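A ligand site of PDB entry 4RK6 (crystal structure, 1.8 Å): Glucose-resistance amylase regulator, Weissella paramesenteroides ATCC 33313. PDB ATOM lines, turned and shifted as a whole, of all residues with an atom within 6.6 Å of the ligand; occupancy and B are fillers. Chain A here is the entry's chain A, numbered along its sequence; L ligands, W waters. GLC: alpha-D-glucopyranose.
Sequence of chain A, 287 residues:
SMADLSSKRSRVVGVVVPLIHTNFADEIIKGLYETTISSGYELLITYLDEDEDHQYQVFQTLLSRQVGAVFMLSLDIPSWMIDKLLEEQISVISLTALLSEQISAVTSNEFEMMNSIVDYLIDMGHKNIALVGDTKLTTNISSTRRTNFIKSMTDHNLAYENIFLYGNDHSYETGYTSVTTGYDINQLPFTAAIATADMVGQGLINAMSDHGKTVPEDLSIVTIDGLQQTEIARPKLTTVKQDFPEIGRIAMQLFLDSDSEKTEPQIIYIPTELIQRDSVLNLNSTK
The side-chain carboxylate (OD1) of Asp 225 lies within hydrogen-bond range of the side-chain amide nitrogen (NE2) of Gln 242, 3.0 Å away.
The backbone carbonyl oxygen (O) of Thr 196 is in hydrogen-bond range of the guanidinium group (NH1) of Arg 145 (2.8 Å).
NE of Arg 145 lies within salt-bridge range of OE1 of Glu 110 (2.9 Å).
OG of Ser 108 lies within hydrogen-bond range of OE1 of Gln 242 (2.6 Å).
OG1 of Thr 196 is in hydrogen-bond range of ND1 of His 170 (2.7 Å).
The backbone NH (N) of Asp 134 lies within hydrogen-bond range of the side-chain hydroxyl (OG1) of Thr 196 (3.0 Å).
O4 of the ligand lies within hydrogen-bond range of OD1 of Asp 225 (2.5 Å).
O of Thr 96 sits at hydrogen-bond distance from O2 of the ligand, at 3.5 Å.
OG1 of Thr 96 is in hydrogen-bond range of O2 of the ligand (2.8 Å).
NH2 of Arg 145 is in hydrogen-bond range of O4 of the ligand, at 2.9 Å.
An oxygen (O6) of the ligand is in hydrogen-bond range of the side-chain hydroxyl (OG1) of Thr 22.
The side-chain amide nitrogen (NE2) of Gln 242 sits at hydrogen-bond distance from an oxygen (O3) of the ligand (3.0 Å).
Merely in contact with the ligand: Phe 24, Thr 196, Ala 197, His 170 and Ile 224.
Hydrophobic or aromatic side chains within 4 Å of the ligand: Phe 24, His 170, Ala 197 and Ile 224.
The nearest printed residue that does not touch the ligand is Glu 110 (4.3 Å).
Water W4 lies within hydrogen-bond range of the backbone carbonyl oxygen of Thr 96 (2.6 Å), an oxygen (O3) of the ligand (2.7 Å) and the side-chain carboxylate of Glu 110 (2.8 Å).
Water W2 bridges O1 of the ligand (2.7 Å) and NE2 of His 170 (3.3 Å).
Water W1 bridges N of Thr 22 (2.9 Å) and O5 of the ligand (3.3 Å).
Water W3 lies within hydrogen-bond range of the backbone carbonyl oxygen of Leu 73 (2.7 Å) and an oxygen (O2) of the ligand (3.3 Å).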
ATOM      1  N   HIS A  21      13.354  22.627  10.602  1.00  0.00           N
ATOM      2  CA  HIS A  21      14.552  23.216  11.214  1.00  0.00           C
ATOM      3  C   HIS A  21      15.821  22.845  10.465  1.00  0.00           C
ATOM      4  O   HIS A  21      15.928  21.733   9.946  1.00  0.00           O
ATOM      5  CB  HIS A  21      14.663  22.765  12.677  1.00  0.00           C
ATOM      6  CG  HIS A  21      14.699  21.276  12.863  1.00  0.00           C
ATOM      7  ND1 HIS A  21      13.586  20.485  12.740  1.00  0.00           N
ATOM      8  CD2 HIS A  21      15.723  20.439  13.169  1.00  0.00           C
ATOM      9  CE1 HIS A  21      13.914  19.225  12.955  1.00  0.00           C
ATOM     10  NE2 HIS A  21      15.202  19.175  13.228  1.00  0.00           N
ATOM     11  N   THR A  22      16.778  23.773  10.434  1.00  0.00           N
ATOM     12  CA  THR A  22      18.149  23.472  10.036  1.00  0.00           C
ATOM     13  C   THR A  22      18.681  22.444  11.066  1.00  0.00           C
ATOM     14  O   THR A  22      18.051  22.208  12.114  1.00  0.00           O
ATOM     15  CB  THR A  22      19.059  24.744  10.013  1.00  0.00           C
ATOM     16  OG1 THR A  22      18.526  25.737   9.107  1.00  0.00           O
ATOM     17  CG2 THR A  22      20.478  24.425   9.586  1.00  0.00           C
ATOM     18  N   ASN A  23      19.835  21.854  10.768  1.00  0.00           N
ATOM     19  CA  ASN A  23      20.517  20.989  11.733  1.00  0.00           C
ATOM     20  C   ASN A  23      21.090  21.696  12.971  1.00  0.00           C
ATOM     21  O   ASN A  23      21.761  21.051  13.790  1.00  0.00           O
ATOM     22  CB  ASN A  23      21.619  20.153  11.061  1.00  0.00           C
ATOM     23  CG  ASN A  23      21.121  18.786  10.602  1.00  0.00           C
ATOM     24  OD1 ASN A  23      20.245  18.182  11.233  1.00  0.00           O
ATOM     25  ND2 ASN A  23      21.690  18.300   9.508  1.00  0.00           N
ATOM     26  N   PHE A  24      20.825  22.995  13.148  1.00  0.00           N
ATOM     27  CA  PHE A  24      21.325  23.663  14.343  1.00  0.00           C
ATOM     28  C   PHE A  24      20.691  23.112  15.610  1.00  0.00           C
ATOM     29  O   PHE A  24      21.334  23.098  16.659  1.00  0.00           O
ATOM     30  CB  PHE A  24      21.235  25.205  14.269  1.00  0.00           C
ATOM     31  CG  PHE A  24      19.888  25.773  14.586  1.00  0.00           C
ATOM     32  CD1 PHE A  24      18.977  26.016  13.573  1.00  0.00           C
ATOM     33  CD2 PHE A  24      19.544  26.128  15.880  1.00  0.00           C
ATOM     34  CE1 PHE A  24      17.725  26.541  13.868  1.00  0.00           C
ATOM     35  CE2 PHE A  24      18.308  26.670  16.179  1.00  0.00           C
ATOM     36  CZ  PHE A  24      17.394  26.880  15.170  1.00  0.00           C
ATOM     37  N   LEU A  73      13.294  27.124  20.750  1.00  0.00           N
ATOM     38  CA  LEU A  73      14.266  27.358  19.671  1.00  0.00           C
ATOM     39  C   LEU A  73      13.683  28.146  18.495  1.00  0.00           C
ATOM     40  O   LEU A  73      14.419  28.812  17.773  1.00  0.00           O
ATOM     41  CB  LEU A  73      14.799  26.040  19.120  1.00  0.00           C
ATOM     42  CG  LEU A  73      15.290  24.962  20.079  1.00  0.00           C
ATOM     43  CD1 LEU A  73      16.295  24.067  19.353  1.00  0.00           C
ATOM     44  CD2 LEU A  73      15.912  25.528  21.341  1.00  0.00           C
ATOM     45  N   LEU A  75      11.240  30.884  16.288  1.00  0.00           N
ATOM     46  CA  LEU A  75      10.906  32.300  16.366  1.00  0.00           C
ATOM     47  C   LEU A  75       9.376  32.445  16.359  1.00  0.00           C
ATOM     48  O   LEU A  75       8.847  33.547  16.524  1.00  0.00           O
ATOM     49  CB  LEU A  75      11.539  33.081  15.213  1.00  0.00           C
ATOM     50  N   LEU A  95      16.209  30.483  22.746  1.00  0.00           N
ATOM     51  CA  LEU A  95      17.548  30.184  22.242  1.00  0.00           C
ATOM     52  C   LEU A  95      17.661  30.564  20.767  1.00  0.00           C
ATOM     53  O   LEU A  95      16.844  30.154  19.956  1.00  0.00           O
ATOM     54  CB  LEU A  95      17.851  28.703  22.442  1.00  0.00           C
ATOM     55  CG  LEU A  95      18.242  28.258  23.861  1.00  0.00           C
ATOM     56  CD1 LEU A  95      17.185  28.490  24.904  1.00  0.00           C
ATOM     57  CD2 LEU A  95      18.573  26.770  23.819  1.00  0.00           C
ATOM     58  N   THR A  96      18.674  31.375  20.467  1.00  0.00           N
ATOM     59  CA  THR A  96      18.983  31.894  19.119  1.00  0.00           C
ATOM     60  C   THR A  96      18.002  32.967  18.662  1.00  0.00           C
ATOM     61  O   THR A  96      18.089  33.470  17.562  1.00  0.00           O
ATOM     62  CB  THR A  96      19.109  30.771  18.046  1.00  0.00           C
ATOM     63  OG1 THR A  96      17.808  30.369  17.586  1.00  0.00           O
ATOM     64  CG2 THR A  96      19.884  29.590  18.572  1.00  0.00           C
ATOM     65  N   ALA A  97      17.125  33.388  19.565  1.00  0.00           N
ATOM     66  CA  ALA A  97      16.075  34.320  19.231  1.00  0.00           C
ATOM     67  C   ALA A  97      15.544  34.917  20.514  1.00  0.00           C
ATOM     68  O   ALA A  97      15.487  34.261  21.541  1.00  0.00           O
ATOM     69  CB  ALA A  97      14.965  33.591  18.477  1.00  0.00           C
ATOM     70  N   THR A 107      21.759  33.705  22.807  1.00  0.00           N
ATOM     71  CA  THR A 107      21.850  33.846  21.354  1.00  0.00           C
ATOM     72  C   THR A 107      23.205  34.362  20.920  1.00  0.00           C
ATOM     73  O   THR A 107      23.915  35.040  21.685  1.00  0.00           O
ATOM     74  CB  THR A 107      20.718  34.778  20.832  1.00  0.00           C
ATOM     75  OG1 THR A 107      20.732  34.861  19.396  1.00  0.00           O
ATOM     76  CG2 THR A 107      20.855  36.199  21.397  1.00  0.00           C
ATOM     77  N   SER A 108      23.574  34.062  19.684  1.00  0.00           N
ATOM     78  CA  SER A 108      24.638  34.813  19.031  1.00  0.00           C
ATOM     79  C   SER A 108      24.105  36.215  18.807  1.00  0.00           C
ATOM     80  O   SER A 108      22.896  36.402  18.603  1.00  0.00           O
ATOM     81  CB  SER A 108      25.032  34.165  17.689  1.00  0.00           C
ATOM     82  OG  SER A 108      25.491  32.820  17.877  1.00  0.00           O
ATOM     83  N   GLU A 110      23.151  38.953  16.604  1.00  0.00           N
ATOM     84  CA  GLU A 110      22.807  38.968  15.170  1.00  0.00           C
ATOM     85  C   GLU A 110      23.452  40.119  14.411  1.00  0.00           C
ATOM     86  O   GLU A 110      23.986  39.917  13.321  1.00  0.00           O
ATOM     87  CB  GLU A 110      21.282  38.963  14.978  1.00  0.00           C
ATOM     88  CG  GLU A 110      20.632  37.614  15.214  1.00  0.00           C
ATOM     89  CD  GLU A 110      20.705  36.685  14.006  1.00  0.00           C
ATOM     90  OE1 GLU A 110      21.128  37.123  12.908  1.00  0.00           O
ATOM     91  OE2 GLU A 110      20.297  35.530  14.156  1.00  0.00           O
ATOM     92  N   MET A 113      27.237  39.425  14.031  1.00  0.00           N
ATOM     93  CA  MET A 113      27.480  38.387  12.994  1.00  0.00           C
ATOM     94  C   MET A 113      27.413  38.999  11.643  1.00  0.00           C
ATOM     95  O   MET A 113      28.374  38.890  10.851  1.00  0.00           O
ATOM     96  CB  MET A 113      26.460  37.247  13.032  1.00  0.00           C
ATOM     97  CG  MET A 113      26.665  36.343  14.238  1.00  0.00           C
ATOM     98  SD  MET A 113      25.699  34.647  13.939  1.00  0.00           S
ATOM     99  CE  MET A 113      23.876  35.332  14.305  1.00  0.00           C
ATOM    100  N   ASP A 134      16.457  33.441   4.172  1.00  0.00           N
ATOM    101  CA  ASP A 134      15.241  33.960   4.799  1.00  0.00           C
ATOM    102  C   ASP A 134      15.340  35.494   4.894  1.00  0.00           C
ATOM    103  O   ASP A 134      15.928  36.035   5.819  1.00  0.00           O
ATOM    104  CB  ASP A 134      15.003  33.275   6.144  1.00  0.00           C
ATOM    105  CG  ASP A 134      13.671  33.647   6.761  1.00  0.00           C
ATOM    106  OD1 ASP A 134      12.987  34.530   6.221  1.00  0.00           O
ATOM    107  OD2 ASP A 134      13.295  33.051   7.785  1.00  0.00           O
ATOM    108  N   ARG A 145      17.793  39.403   9.871  1.00  0.00           N
ATOM    109  CA  ARG A 145      18.976  39.439   9.004  1.00  0.00           C
ATOM    110  C   ARG A 145      18.875  40.425   7.864  1.00  0.00           C
ATOM    111  O   ARG A 145      19.832  41.111   7.556  1.00  0.00           O
ATOM    112  CB  ARG A 145      19.318  38.039   8.527  1.00  0.00           C
ATOM    113  CG  ARG A 145      19.768  37.230   9.734  1.00  0.00           C
ATOM    114  CD  ARG A 145      20.316  35.839   9.444  1.00  0.00           C
ATOM    115  NE  ARG A 145      20.762  35.309  10.733  1.00  0.00           N
ATOM    116  CZ  ARG A 145      21.038  34.034  10.981  1.00  0.00           C
ATOM    117  NH1 ARG A 145      20.973  33.108  10.028  1.00  0.00           N
ATOM    118  NH2 ARG A 145      21.381  33.688  12.223  1.00  0.00           N
ATOM    119  N   HIS A 170      15.469  29.110   4.595  1.00  0.00           N
ATOM    120  CA  HIS A 170      16.888  28.766   4.717  1.00  0.00           C
ATOM    121  C   HIS A 170      17.244  27.498   3.936  1.00  0.00           C
ATOM    122  O   HIS A 170      18.238  26.824   4.279  1.00  0.00           O
ATOM    123  CB  HIS A 170      17.234  28.490   6.188  1.00  0.00           C
ATOM    124  CG  HIS A 170      17.060  29.649   7.097  1.00  0.00           C
ATOM    125  ND1 HIS A 170      17.831  30.785   7.008  1.00  0.00           N
ATOM    126  CD2 HIS A 170      16.247  29.828   8.160  1.00  0.00           C
ATOM    127  CE1 HIS A 170      17.480  31.632   7.953  1.00  0.00           C
ATOM    128  NE2 HIS A 170      16.512  31.076   8.662  1.00  0.00           N
ATOM    129  N   THR A 196      21.928  32.883   4.477  1.00  0.00           N
ATOM    130  CA  THR A 196      21.432  32.928   5.855  1.00  0.00           C
ATOM    131  C   THR A 196      21.517  31.579   6.588  1.00  0.00           C
ATOM    132  O   THR A 196      21.292  31.514   7.799  1.00  0.00           O
ATOM    133  CB  THR A 196      19.953  33.415   5.952  1.00  0.00           C
ATOM    134  OG1 THR A 196      19.084  32.479   5.289  1.00  0.00           O
ATOM    135  CG2 THR A 196      19.819  34.769   5.377  1.00  0.00           C
ATOM    136  N   ALA A 197      21.828  30.520   5.841  1.00  0.00           N
ATOM    137  CA  ALA A 197      22.114  29.210   6.446  1.00  0.00           C
ATOM    138  C   ALA A 197      23.056  28.463   5.554  1.00  0.00           C
ATOM    139  O   ALA A 197      23.179  28.770   4.362  1.00  0.00           O
ATOM    140  CB  ALA A 197      20.855  28.426   6.678  1.00  0.00           C
ATOM    141  N   ASP A 198      23.790  27.503   6.120  1.00  0.00           N
ATOM    142  CA  ASP A 198      24.778  26.759   5.346  1.00  0.00           C
ATOM    143  C   ASP A 198      24.224  26.118   4.045  1.00  0.00           C
ATOM    144  O   ASP A 198      24.880  26.162   2.991  1.00  0.00           O
ATOM    145  CB  ASP A 198      25.426  25.651   6.178  1.00  0.00           C
ATOM    146  CG  ASP A 198      26.107  26.195   7.432  1.00  0.00           C
ATOM    147  OD1 ASP A 198      26.630  27.337   7.440  1.00  0.00           O
ATOM    148  OD2 ASP A 198      26.100  25.425   8.410  1.00  0.00           O
ATOM    149  N   ILE A 224      26.060  31.662   7.246  1.00  0.00           N
ATOM    150  CA  ILE A 224      25.852  31.755   8.677  1.00  0.00           C
ATOM    151  C   ILE A 224      25.460  30.399   9.221  1.00  0.00           C
ATOM    152  O   ILE A 224      24.509  29.797   8.732  1.00  0.00           O
ATOM    153  CB  ILE A 224      24.767  32.776   9.033  1.00  0.00           C
ATOM    154  CG1 ILE A 224      25.275  34.163   8.672  1.00  0.00           C
ATOM    155  CG2 ILE A 224      24.432  32.661  10.524  1.00  0.00           C
ATOM    156  CD1 ILE A 224      24.213  35.229   8.661  1.00  0.00           C
ATOM    157  N   ASP A 225      26.229  29.927  10.211  1.00  0.00           N
ATOM    158  CA  ASP A 225      25.972  28.790  11.099  1.00  0.00           C
ATOM    159  C   ASP A 225      27.267  27.985  11.296  1.00  0.00           C
ATOM    160  O   ASP A 225      27.641  27.673  12.413  1.00  0.00           O
ATOM    161  CB  ASP A 225      24.860  27.828  10.650  1.00  0.00           C
ATOM    162  CG  ASP A 225      23.469  28.377  10.899  1.00  0.00           C
ATOM    163  OD1 ASP A 225      23.344  29.439  11.552  1.00  0.00           O
ATOM    164  OD2 ASP A 225      22.499  27.756  10.392  1.00  0.00           O
ATOM    165  N   LEU A 227      28.003  24.800  10.316  1.00  0.00           N
ATOM    166  CA  LEU A 227      27.843  23.354  10.557  1.00  0.00           C
ATOM    167  C   LEU A 227      28.540  22.509   9.466  1.00  0.00           C
ATOM    168  O   LEU A 227      29.236  23.056   8.594  1.00  0.00           O
ATOM    169  CB  LEU A 227      26.378  23.015  10.739  1.00  0.00           C
ATOM    170  CG  LEU A 227      25.728  23.685  11.979  1.00  0.00           C
ATOM    171  CD1 LEU A 227      24.224  23.537  11.904  1.00  0.00           C
ATOM    172  CD2 LEU A 227      26.290  23.121  13.265  1.00  0.00           C
ATOM    173  N   GLN A 242      28.474  29.636  14.601  1.00  0.00           N
ATOM    174  CA  GLN A 242      27.817  29.812  15.912  1.00  0.00           C
ATOM    175  C   GLN A 242      28.219  28.680  16.837  1.00  0.00           C
ATOM    176  O   GLN A 242      28.406  27.527  16.403  1.00  0.00           O
ATOM    177  CB  GLN A 242      26.301  29.814  15.768  1.00  0.00           C
ATOM    178  CG  GLN A 242      25.787  30.873  14.813  1.00  0.00           C
ATOM    179  CD  GLN A 242      24.316  31.195  15.079  1.00  0.00           C
ATOM    180  OE1 GLN A 242      23.949  31.550  16.183  1.00  0.00           O
ATOM    181  NE2 GLN A 242      23.473  30.996  14.081  1.00  0.00           N
ATOM    182  N   PHE A 244      26.638  26.570  18.893  1.00  0.00           N
ATOM    183  CA  PHE A 244      25.308  26.080  19.288  1.00  0.00           C
ATOM    184  C   PHE A 244      25.350  25.286  20.592  1.00  0.00           C
ATOM    185  O   PHE A 244      24.466  25.424  21.428  1.00  0.00           O
ATOM    186  CB  PHE A 244      24.640  25.266  18.185  1.00  0.00           C
ATOM    187  CG  PHE A 244      24.257  26.077  16.982  1.00  0.00           C
ATOM    188  CD1 PHE A 244      23.323  27.100  17.081  1.00  0.00           C
ATOM    189  CD2 PHE A 244      24.863  25.848  15.749  1.00  0.00           C
ATOM    190  CE1 PHE A 244      22.990  27.873  15.979  1.00  0.00           C
ATOM    191  CE2 PHE A 244      24.537  26.622  14.638  1.00  0.00           C
ATOM    192  CZ  PHE A 244      23.587  27.630  14.761  1.00  0.00           C
HETATM  193  C1  GLC L   1      17.390  29.808  13.008  1.00  0.00           C
HETATM  194  C2  GLC L   1      18.358  30.360  14.055  1.00  0.00           C
HETATM  195  C3  GLC L   1      19.541  31.081  13.441  1.00  0.00           C
HETATM  196  C4  GLC L   1      20.137  30.241  12.319  1.00  0.00           C
HETATM  197  C5  GLC L   1      19.050  30.039  11.262  1.00  0.00           C
HETATM  198  C6  GLC L   1      19.540  29.171  10.098  1.00  0.00           C
HETATM  199  O1  GLC L   1      16.570  30.846  12.624  1.00  0.00           O
HETATM  200  O2  GLC L   1      17.691  31.283  14.910  1.00  0.00           O
HETATM  201  O3  GLC L   1      20.474  31.252  14.509  1.00  0.00           O
HETATM  202  O4  GLC L   1      21.272  30.857  11.802  1.00  0.00           O
HETATM  203  O5  GLC L   1      17.961  29.335  11.798  1.00  0.00           O
HETATM  204  O6  GLC L   1      19.912  27.899  10.532  1.00  0.00           O
HETATM  205  O   HOH W   1      16.343  26.640  10.844  1.00  0.00           O
HETATM  206  O   HOH W   2      14.362  30.377  11.114  1.00  0.00           O
HETATM  207  O   HOH W   3      14.636  30.193  15.438  1.00  0.00           O
HETATM  208  O   HOH W   4      20.223  33.496  16.009  1.00  0.00           O
